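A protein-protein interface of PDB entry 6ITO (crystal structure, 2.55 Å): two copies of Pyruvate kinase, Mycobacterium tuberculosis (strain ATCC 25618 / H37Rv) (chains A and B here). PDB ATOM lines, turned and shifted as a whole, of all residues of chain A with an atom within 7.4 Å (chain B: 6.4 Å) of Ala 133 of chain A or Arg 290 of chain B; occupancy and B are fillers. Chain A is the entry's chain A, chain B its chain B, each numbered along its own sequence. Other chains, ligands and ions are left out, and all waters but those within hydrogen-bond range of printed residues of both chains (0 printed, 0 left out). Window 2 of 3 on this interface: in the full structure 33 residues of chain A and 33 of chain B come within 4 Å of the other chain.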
ATOM      1  N   TRP A  88      15.662   9.115  33.217  1.00  0.00           N
ATOM      2  CA  TRP A  88      14.744   9.868  32.333  1.00  0.00           C
ATOM      3  C   TRP A  88      13.563   8.949  31.954  1.00  0.00           C
ATOM      4  O   TRP A  88      13.764   8.016  31.116  1.00  0.00           O
ATOM      5  CB  TRP A  88      15.504  10.433  31.107  1.00  0.00           C
ATOM      6  CG  TRP A  88      16.298  11.685  31.396  1.00  0.00           C
ATOM      7  CD1 TRP A  88      16.276  12.426  32.549  1.00  0.00           C
ATOM      8  CD2 TRP A  88      17.179  12.391  30.491  1.00  0.00           C
ATOM      9  NE1 TRP A  88      17.103  13.512  32.439  1.00  0.00           N
ATOM     10  CE2 TRP A  88      17.671  13.519  31.189  1.00  0.00           C
ATOM     11  CE3 TRP A  88      17.613  12.175  29.176  1.00  0.00           C
ATOM     12  CZ2 TRP A  88      18.542  14.439  30.599  1.00  0.00           C
ATOM     13  CZ3 TRP A  88      18.499  13.067  28.610  1.00  0.00           C
ATOM     14  CH2 TRP A  88      18.948  14.187  29.310  1.00  0.00           C
ATOM     15  N   GLU A  90       9.830   7.940  30.506  1.00  0.00           N
ATOM     16  CA  GLU A  90       8.827   8.211  29.437  1.00  0.00           C
ATOM     17  C   GLU A  90       7.723   9.097  30.026  1.00  0.00           C
ATOM     18  O   GLU A  90       7.069   8.657  30.973  1.00  0.00           O
ATOM     19  CB  GLU A  90       8.275   6.891  28.891  1.00  0.00           C
ATOM     20  CG  GLU A  90       7.208   7.058  27.821  1.00  0.00           C
ATOM     21  CD  GLU A  90       6.758   5.749  27.170  1.00  0.00           C
ATOM     22  OE1 GLU A  90       7.594   4.845  27.058  1.00  0.00           O
ATOM     23  OE2 GLU A  90       5.548   5.630  26.788  1.00  0.00           O
ATOM     24  N   ARG A 124      14.163  15.674  17.105  1.00  0.00           N
ATOM     25  CA  ARG A 124      14.357  14.432  17.886  1.00  0.00           C
ATOM     26  C   ARG A 124      15.769  14.421  18.476  1.00  0.00           C
ATOM     27  O   ARG A 124      16.663  15.059  17.894  1.00  0.00           O
ATOM     28  CB  ARG A 124      14.055  13.224  17.002  1.00  0.00           C
ATOM     29  CG  ARG A 124      12.598  13.170  16.577  1.00  0.00           C
ATOM     30  CD  ARG A 124      12.244  12.064  15.619  1.00  0.00           C
ATOM     31  NE  ARG A 124      11.016  11.403  16.062  1.00  0.00           N
ATOM     32  CZ  ARG A 124       9.785  11.948  16.034  1.00  0.00           C
ATOM     33  NH1 ARG A 124       9.598  13.174  15.554  1.00  0.00           N
ATOM     34  NH2 ARG A 124       8.748  11.253  16.483  1.00  0.00           N
ATOM     35  N   VAL A 125      15.923  13.794  19.642  1.00  0.00           N
ATOM     36  CA  VAL A 125      17.212  13.658  20.386  1.00  0.00           C
ATOM     37  C   VAL A 125      17.391  12.192  20.768  1.00  0.00           C
ATOM     38  O   VAL A 125      16.670  11.738  21.663  1.00  0.00           O
ATOM     39  CB  VAL A 125      17.245  14.555  21.639  1.00  0.00           C
ATOM     40  CG1 VAL A 125      18.571  14.453  22.363  1.00  0.00           C
ATOM     41  CG2 VAL A 125      16.930  16.009  21.315  1.00  0.00           C
ATOM     42  N   LEU A 126      18.329  11.490  20.126  1.00  0.00           N
ATOM     43  CA  LEU A 126      18.693  10.099  20.482  1.00  0.00           C
ATOM     44  C   LEU A 126      19.930  10.124  21.378  1.00  0.00           C
ATOM     45  O   LEU A 126      20.844  10.886  21.092  1.00  0.00           O
ATOM     46  CB  LEU A 126      18.915   9.291  19.206  1.00  0.00           C
ATOM     47  CG  LEU A 126      17.776   9.360  18.185  1.00  0.00           C
ATOM     48  CD1 LEU A 126      17.685   8.076  17.371  1.00  0.00           C
ATOM     49  CD2 LEU A 126      16.447   9.644  18.864  1.00  0.00           C
ATOM     50  N   VAL A 127      19.892   9.369  22.473  1.00  0.00           N
ATOM     51  CA  VAL A 127      20.965   9.297  23.505  1.00  0.00           C
ATOM     52  C   VAL A 127      21.617   7.924  23.400  1.00  0.00           C
ATOM     53  O   VAL A 127      20.891   6.971  23.087  1.00  0.00           O
ATOM     54  CB  VAL A 127      20.392   9.532  24.917  1.00  0.00           C
ATOM     55  CG1 VAL A 127      21.464   9.406  25.998  1.00  0.00           C
ATOM     56  CG2 VAL A 127      19.677  10.867  25.020  1.00  0.00           C
ATOM     57  N   ASP A 129      23.401   6.239  21.365  1.00  0.00           N
ATOM     58  CA  ASP A 129      23.206   5.554  20.037  1.00  0.00           C
ATOM     59  C   ASP A 129      21.771   4.952  19.929  1.00  0.00           C
ATOM     60  O   ASP A 129      21.621   3.910  19.209  1.00  0.00           O
ATOM     61  CB  ASP A 129      24.289   4.473  19.781  1.00  0.00           C
ATOM     62  CG  ASP A 129      25.703   5.008  19.502  1.00  0.00           C
ATOM     63  OD1 ASP A 129      25.849   6.244  19.339  1.00  0.00           O
ATOM     64  OD2 ASP A 129      26.661   4.178  19.467  1.00  0.00           O
ATOM     65  N   GLY A 130      20.750   5.571  20.590  1.00  0.00           N
ATOM     66  CA  GLY A 130      19.307   5.434  20.220  1.00  0.00           C
ATOM     67  C   GLY A 130      18.353   5.118  21.402  1.00  0.00           C
ATOM     68  O   GLY A 130      17.141   5.361  21.242  1.00  0.00           O
ATOM     69  N   LYS A 131      18.862   4.587  22.526  1.00  0.00           N
ATOM     70  CA  LYS A 131      18.056   3.831  23.547  1.00  0.00           C
ATOM     71  C   LYS A 131      17.084   4.766  24.281  1.00  0.00           C
ATOM     72  O   LYS A 131      15.994   4.322  24.580  1.00  0.00           O
ATOM     73  CB  LYS A 131      18.960   3.141  24.565  1.00  0.00           C
ATOM     74  CG  LYS A 131      20.402   2.907  24.117  1.00  0.00           C
ATOM     75  CD  LYS A 131      20.526   2.183  22.784  1.00  0.00           C
ATOM     76  CE  LYS A 131      21.923   1.653  22.525  1.00  0.00           C
ATOM     77  NZ  LYS A 131      22.404   0.795  23.636  1.00  0.00           N
ATOM     78  N   VAL A 132      17.518   5.968  24.650  1.00  0.00           N
ATOM     79  CA  VAL A 132      16.645   7.032  25.247  1.00  0.00           C
ATOM     80  C   VAL A 132      16.410   8.124  24.196  1.00  0.00           C
ATOM     81  O   VAL A 132      17.402   8.688  23.697  1.00  0.00           O
ATOM     82  CB  VAL A 132      17.269   7.613  26.529  1.00  0.00           C
ATOM     83  CG1 VAL A 132      16.611   8.930  26.953  1.00  0.00           C
ATOM     84  CG2 VAL A 132      17.234   6.600  27.657  1.00  0.00           C
ATOM     85  N   ALA A 133      15.142   8.399  23.873  1.00  0.00           N
ATOM     86  CA  ALA A 133      14.720   9.318  22.785  1.00  0.00           C
ATOM     87  C   ALA A 133      13.842  10.422  23.358  1.00  0.00           C
ATOM     88  O   ALA A 133      12.950  10.115  24.142  1.00  0.00           O
ATOM     89  CB  ALA A 133      14.006   8.551  21.707  1.00  0.00           C
ATOM     90  N   LEU A 134      14.128  11.668  23.003  1.00  0.00           N
ATOM     91  CA  LEU A 134      13.322  12.845  23.391  1.00  0.00           C
ATOM     92  C   LEU A 134      12.793  13.517  22.137  1.00  0.00           C
ATOM     93  O   LEU A 134      13.326  13.250  21.053  1.00  0.00           O
ATOM     94  CB  LEU A 134      14.173  13.828  24.205  1.00  0.00           C
ATOM     95  CG  LEU A 134      15.266  13.216  25.081  1.00  0.00           C
ATOM     96  CD1 LEU A 134      16.108  14.309  25.720  1.00  0.00           C
ATOM     97  CD2 LEU A 134      14.680  12.313  26.142  1.00  0.00           C
ATOM     98  N   VAL A 135      11.805  14.385  22.304  1.00  0.00           N
ATOM     99  CA  VAL A 135      11.366  15.353  21.276  1.00  0.00           C
ATOM    100  C   VAL A 135      11.439  16.747  21.876  1.00  0.00           C
ATOM    101  O   VAL A 135      11.097  16.898  23.054  1.00  0.00           O
ATOM    102  CB  VAL A 135       9.957  15.019  20.759  1.00  0.00           C
ATOM    103  CG1 VAL A 135       9.455  16.063  19.781  1.00  0.00           C
ATOM    104  CG2 VAL A 135       9.906  13.626  20.136  1.00  0.00           C
ATOM    105  N   CYS A 146      12.460  19.503  26.389  1.00  0.00           N
ATOM    106  CA  CYS A 146      12.173  18.271  25.622  1.00  0.00           C
ATOM    107  C   CYS A 146      11.249  17.377  26.431  1.00  0.00           C
ATOM    108  O   CYS A 146      11.183  17.562  27.644  1.00  0.00           O
ATOM    109  CB  CYS A 146      13.456  17.514  25.290  1.00  0.00           C
ATOM    110  SG  CYS A 146      14.812  18.591  24.757  1.00  0.00           S
ATOM    111  N   THR A 147      10.596  16.429  25.773  1.00  0.00           N
ATOM    112  CA  THR A 147       9.742  15.407  26.407  1.00  0.00           C
ATOM    113  C   THR A 147      10.328  14.048  26.110  1.00  0.00           C
ATOM    114  O   THR A 147      10.491  13.735  24.936  1.00  0.00           O
ATOM    115  CB  THR A 147       8.294  15.492  25.910  1.00  0.00           C
ATOM    116  OG1 THR A 147       7.914  16.866  25.789  1.00  0.00           O
ATOM    117  CG2 THR A 147       7.338  14.763  26.820  1.00  0.00           C
ATOM    118  N   VAL A 148      10.649  13.289  27.140  1.00  0.00           N
ATOM    119  CA  VAL A 148      11.148  11.893  27.004  1.00  0.00           C
ATOM    120  C   VAL A 148      10.046  11.055  26.354  1.00  0.00           C
ATOM    121  O   VAL A 148       8.952  10.990  26.926  1.00  0.00           O
ATOM    122  CB  VAL A 148      11.574  11.306  28.363  1.00  0.00           C
ATOM    123  CG1 VAL A 148      12.156   9.900  28.211  1.00  0.00           C
ATOM    124  CG2 VAL A 148      12.548  12.223  29.101  1.00  0.00           C
ATOM    125  N   VAL A 149      10.323  10.486  25.186  1.00  0.00           N
ATOM    126  CA  VAL A 149       9.345   9.703  24.378  1.00  0.00           C
ATOM    127  C   VAL A 149       9.694   8.220  24.494  1.00  0.00           C
ATOM    128  O   VAL A 149       8.796   7.409  24.451  1.00  0.00           O
ATOM    129  CB  VAL A 149       9.311  10.184  22.911  1.00  0.00           C
ATOM    130  CG1 VAL A 149       8.674   9.158  21.982  1.00  0.00           C
ATOM    131  CG2 VAL A 149       8.593  11.514  22.785  1.00  0.00           C
ATOM    132  N   GLU A 150      10.968   7.904  24.611  1.00  0.00           N
ATOM    133  CA  GLU A 150      11.464   6.570  25.040  1.00  0.00           C
ATOM    134  C   GLU A 150      12.347   6.770  26.287  1.00  0.00           C
ATOM    135  O   GLU A 150      13.301   7.581  26.219  1.00  0.00           O
ATOM    136  CB  GLU A 150      12.225   5.891  23.892  1.00  0.00           C
ATOM    137  CG  GLU A 150      11.399   4.898  23.071  1.00  0.00           C
ATOM    138  CD  GLU A 150      11.611   5.008  21.561  1.00  0.00           C
ATOM    139  OE1 GLU A 150      10.971   5.878  20.950  1.00  0.00           O
ATOM    140  OE2 GLU A 150      12.448   4.245  21.006  1.00  0.00           O
ATOM    141  N   GLY A 151      12.009   6.095  27.386  1.00  0.00           N
ATOM    142  CA  GLY A 151      12.580   6.348  28.726  1.00  0.00           C
ATOM    143  C   GLY A 151      13.758   5.445  29.022  1.00  0.00           C
ATOM    144  O   GLY A 151      13.838   4.354  28.401  1.00  0.00           O
ATOM    145  N   GLY A 152      14.644   5.876  29.922  1.00  0.00           N
ATOM    146  CA  GLY A 152      15.840   5.103  30.313  1.00  0.00           C
ATOM    147  C   GLY A 152      16.849   5.920  31.122  1.00  0.00           C
ATOM    148  O   GLY A 152      16.591   7.074  31.493  1.00  0.00           O
ATOM    149  N   GLY A 249      23.516   4.935  11.934  1.00  0.00           N
ATOM    150  CA  GLY A 249      22.195   4.333  12.113  1.00  0.00           C
ATOM    151  C   GLY A 249      21.280   5.173  12.993  1.00  0.00           C
ATOM    152  O   GLY A 249      20.164   4.733  13.215  1.00  0.00           O
ATOM    153  N   VAL A 250      21.743   6.322  13.500  1.00  0.00           N
ATOM    154  CA  VAL A 250      20.863   7.326  14.184  1.00  0.00           C
ATOM    155  C   VAL A 250      20.822   8.618  13.351  1.00  0.00           C
ATOM    156  O   VAL A 250      19.801   9.263  13.356  1.00  0.00           O
ATOM    157  CB  VAL A 250      21.293   7.583  15.642  1.00  0.00           C
ATOM    158  CG1 VAL A 250      21.214   6.325  16.480  1.00  0.00           C
ATOM    159  CG2 VAL A 250      22.674   8.180  15.733  1.00  0.00           C
ATOM    160  N   LEU A 254      17.835   3.862  10.280  1.00  0.00           N
ATOM    161  CA  LEU A 254      18.659   2.660  10.538  1.00  0.00           C
ATOM    162  C   LEU A 254      18.431   1.652   9.412  1.00  0.00           C
ATOM    163  O   LEU A 254      19.317   0.857   9.156  1.00  0.00           O
ATOM    164  CB  LEU A 254      18.321   2.082  11.920  1.00  0.00           C
ATOM    165  CG  LEU A 254      16.926   1.483  12.093  1.00  0.00           C
ATOM    166  CD1 LEU A 254      16.855   0.081  11.506  1.00  0.00           C
ATOM    167  CD2 LEU A 254      16.539   1.455  13.557  1.00  0.00           C
ATOM    168  N   SER B 284      17.158  -8.369  19.642  1.00  0.00           N
ATOM    169  CA  SER B 284      17.409  -7.331  20.680  1.00  0.00           C
ATOM    170  C   SER B 284      16.138  -6.496  20.920  1.00  0.00           C
ATOM    171  O   SER B 284      16.084  -5.805  21.941  1.00  0.00           O
ATOM    172  CB  SER B 284      18.606  -6.472  20.338  1.00  0.00           C
ATOM    173  OG  SER B 284      18.245  -5.362  19.541  1.00  0.00           O
ATOM    174  N   MET B 285      15.130  -6.610  20.045  1.00  0.00           N
ATOM    175  CA  MET B 285      13.876  -5.817  20.141  1.00  0.00           C
ATOM    176  C   MET B 285      12.900  -6.485  21.126  1.00  0.00           C
ATOM    177  O   MET B 285      11.896  -5.861  21.462  1.00  0.00           O
ATOM    178  CB  MET B 285      13.217  -5.661  18.779  1.00  0.00           C
ATOM    179  CG  MET B 285      14.045  -4.825  17.830  1.00  0.00           C
ATOM    180  SD  MET B 285      13.071  -4.112  16.496  1.00  0.00           S
ATOM    181  CE  MET B 285      12.033  -2.990  17.435  1.00  0.00           C
ATOM    182  N   ASN B 288      14.434  -3.975  23.579  1.00  0.00           N
ATOM    183  CA  ASN B 288      14.797  -2.610  23.105  1.00  0.00           C
ATOM    184  C   ASN B 288      13.880  -2.196  21.955  1.00  0.00           C
ATOM    185  O   ASN B 288      13.448  -3.076  21.201  1.00  0.00           O
ATOM    186  CB  ASN B 288      16.267  -2.534  22.689  1.00  0.00           C
ATOM    187  CG  ASN B 288      17.199  -3.004  23.778  1.00  0.00           C
ATOM    188  OD1 ASN B 288      17.243  -2.420  24.859  1.00  0.00           O
ATOM    189  ND2 ASN B 288      17.894  -4.100  23.532  1.00  0.00           N
ATOM    190  N   SER B 289      13.641  -0.889  21.808  1.00  0.00           N
ATOM    191  CA  SER B 289      12.657  -0.302  20.858  1.00  0.00           C
ATOM    192  C   SER B 289      13.271  -0.197  19.449  1.00  0.00           C
ATOM    193  O   SER B 289      12.500  -0.080  18.483  1.00  0.00           O
ATOM    194  CB  SER B 289      12.161   1.034  21.354  1.00  0.00           C
ATOM    195  OG  SER B 289      13.236   1.926  21.561  1.00  0.00           O
ATOM    196  N   ARG B 290      14.601  -0.229  19.355  1.00  0.00           N
ATOM    197  CA  ARG B 290      15.360  -0.269  18.082  1.00  0.00           C
ATOM    198  C   ARG B 290      16.250  -1.500  18.078  1.00  0.00           C
ATOM    199  O   ARG B 290      16.716  -1.943  19.122  1.00  0.00           O
ATOM    200  CB  ARG B 290      16.232   0.970  17.926  1.00  0.00           C
ATOM    201  CG  ARG B 290      15.467   2.261  17.708  1.00  0.00           C
ATOM    202  CD  ARG B 290      16.206   3.479  18.271  1.00  0.00           C
ATOM    203  NE  ARG B 290      15.256   4.482  18.741  1.00  0.00           N
ATOM    204  CZ  ARG B 290      14.671   5.394  17.963  1.00  0.00           C
ATOM    205  NH1 ARG B 290      14.986   5.477  16.675  1.00  0.00           N
ATOM    206  NH2 ARG B 290      13.790   6.234  18.480  1.00  0.00           N
ATOM    207  N   PRO B 291      16.539  -2.069  16.900  1.00  0.00           N
ATOM    208  CA  PRO B 291      17.422  -3.228  16.803  1.00  0.00           C
ATOM    209  C   PRO B 291      18.919  -2.862  16.720  1.00  0.00           C
ATOM    210  O   PRO B 291      19.245  -1.699  16.707  1.00  0.00           O
ATOM    211  CB  PRO B 291      16.931  -3.869  15.498  1.00  0.00           C
ATOM    212  CG  PRO B 291      16.560  -2.681  14.644  1.00  0.00           C
ATOM    213  CD  PRO B 291      16.020  -1.645  15.610  1.00  0.00           C
ATOM    214  N   THR B 292      19.781  -3.864  16.645  1.00  0.00           N
ATOM    215  CA  THR B 292      21.240  -3.698  16.405  1.00  0.00           C
ATOM    216  C   THR B 292      21.481  -3.484  14.905  1.00  0.00           C
ATOM    217  O   THR B 292      20.567  -3.752  14.096  1.00  0.00           O
ATOM    218  CB  THR B 292      22.046  -4.882  16.958  1.00  0.00           C
ATOM    219  OG1 THR B 292      21.744  -6.047  16.190  1.00  0.00           O
ATOM    220  CG2 THR B 292      21.760  -5.154  18.417  1.00  0.00           C
ATOM    221  N   ARG B 293      22.646  -2.974  14.559  1.00  0.00           N
ATOM    222  CA  ARG B 293      23.046  -2.751  13.162  1.00  0.00           C
ATOM    223  C   ARG B 293      23.171  -4.111  12.475  1.00  0.00           C
ATOM    224  O   ARG B 293      22.822  -4.205  11.303  1.00  0.00           O
ATOM    225  CB  ARG B 293      24.341  -1.951  13.120  1.00  0.00           C
ATOM    226  CG  ARG B 293      24.266  -0.642  13.875  1.00  0.00           C
ATOM    227  CD  ARG B 293      23.419   0.370  13.170  1.00  0.00           C
ATOM    228  NE  ARG B 293      23.292   1.555  13.975  1.00  0.00           N
ATOM    229  CZ  ARG B 293      22.358   1.740  14.891  1.00  0.00           C
ATOM    230  NH1 ARG B 293      21.428   0.820  15.087  1.00  0.00           N
ATOM    231  NH2 ARG B 293      22.341   2.855  15.594  1.00  0.00           N
ATOM    232  N   GLU B 295      21.311  -6.712  13.201  1.00  0.00           N
ATOM    233  CA  GLU B 295      19.921  -7.167  13.031  1.00  0.00           C
ATOM    234  C   GLU B 295      19.337  -6.505  11.784  1.00  0.00           C
ATOM    235  O   GLU B 295      18.936  -7.230  10.886  1.00  0.00           O
ATOM    236  CB  GLU B 295      19.134  -6.899  14.311  1.00  0.00           C
ATOM    237  CG  GLU B 295      19.445  -7.916  15.397  1.00  0.00           C
ATOM    238  CD  GLU B 295      19.077  -7.512  16.799  1.00  0.00           C
ATOM    239  OE1 GLU B 295      18.606  -6.368  16.998  1.00  0.00           O
ATOM    240  OE2 GLU B 295      19.274  -8.338  17.689  1.00  0.00           O
ATOM    241  N   TYR B 321       8.083  -5.205  22.572  1.00  0.00           N
ATOM    242  CA  TYR B 321       7.796  -4.324  21.413  1.00  0.00           C
ATOM    243  C   TYR B 321       7.390  -5.155  20.208  1.00  0.00           C
ATOM    244  O   TYR B 321       7.956  -4.997  19.126  1.00  0.00           O
ATOM    245  CB  TYR B 321       8.999  -3.444  21.089  1.00  0.00           C
ATOM    246  CG  TYR B 321       9.493  -2.585  22.226  1.00  0.00           C
ATOM    247  CD1 TYR B 321       8.961  -1.325  22.464  1.00  0.00           C
ATOM    248  CD2 TYR B 321      10.532  -3.012  23.037  1.00  0.00           C
ATOM    249  CE1 TYR B 321       9.456  -0.514  23.473  1.00  0.00           C
ATOM    250  CE2 TYR B 321      11.031  -2.215  24.052  1.00  0.00           C
ATOM    251  CZ  TYR B 321      10.498  -0.963  24.263  1.00  0.00           C
ATOM    252  OH  TYR B 321      11.002  -0.193  25.249  1.00  0.00           O
ATOM    253  N   THR B 328       9.287  -2.323  12.323  1.00  0.00           N
ATOM    254  CA  THR B 328      10.732  -2.166  12.037  1.00  0.00           C
ATOM    255  C   THR B 328      11.124  -3.134  10.915  1.00  0.00           C
ATOM    256  O   THR B 328      11.808  -2.699   9.972  1.00  0.00           O
ATOM    257  CB  THR B 328      11.606  -2.381  13.278  1.00  0.00           C
ATOM    258  OG1 THR B 328      11.386  -1.322  14.203  1.00  0.00           O
ATOM    259  CG2 THR B 328      13.079  -2.416  12.944  1.00  0.00           C
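The guanidinium group of Arg 290 of chain B is in hydrogen-bond range of the backbone carbonyl oxygen of Gly 130 of chain A (3.3 Å). OG of Ser 289 of chain B lies within hydrogen-bond range of OE2 of Glu 150 of chain A. OE2 of Glu 150 of chain A is in salt-bridge range of NH2 of Arg 290 of chain B (3.5 Å).
The backbone carbonyl oxygen of Ala 133 of chain A is in hydrogen-bond range of the backbone NH of Val 149 of chain A, at 2.9 Å. O of Ala 133 of chain A sits at hydrogen-bond distance from N of Glu 150 of chain A, at 3.0 Å.
Leu 126 of chain A touches Arg 290 of chain B. NH2 of Arg 293 of chain B touches O of Asp 129 of chain A, at 3.8 Å. Ala 133 of chain A touches Arg 290 of chain B (CB to NH2, 3.98 Å). Arg 293 of chain B touches Gly 249 of chain A. NH2 of Arg 293 of chain B touches CG1 of Val 250 of chain A, at 3.8 Å. Leu 254 of chain A touches Pro 291 of chain B.
Ala 133 of chain A touches one residue of chain B. Of chain A, only Leu 126 (3.8 Å), Gly 130 (3.3 Å), Ala 133 (3.98 Å) and Glu 150 (3.5 Å) come within 4 Å of Arg 290 of chain B. Of the printed residues of chain B, Glu 150 of chain A touches Ser 289 and Arg 290. Printed residues of chain B within 4 Å of Gly 130 of chain A: Arg 290 (3.3 Å). The nearest printed residue of chain B that does not touch Ala 133 of chain A is Ser 289 of chain B (6.7 Å). The nearest residue of chain A that does not touch Arg 290 of chain B is Leu 254 of chain A (4.4 Å). The nearest printed residue of chain B that does not touch Val 250 of chain A is Arg 290 of chain B (6.0 Å).
Printed residues of chain B that touch a printed residue of chain A: Ser 289, Arg 290, Pro 291 and Arg 293. Among the printed residues, 9 pairs touch across the chains. Among the printed residues, Asp or Glu carboxylates within 4 Å of a Lys or Arg side-chain nitrogen of the other chain: Glu 150 of chain A with Arg 290 of chain B (3.5 Å).
No position is printed for both chains. Of the 9 pairs that touch across the chains among the printed residues, none has its exchanged pair printed and touching as well.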
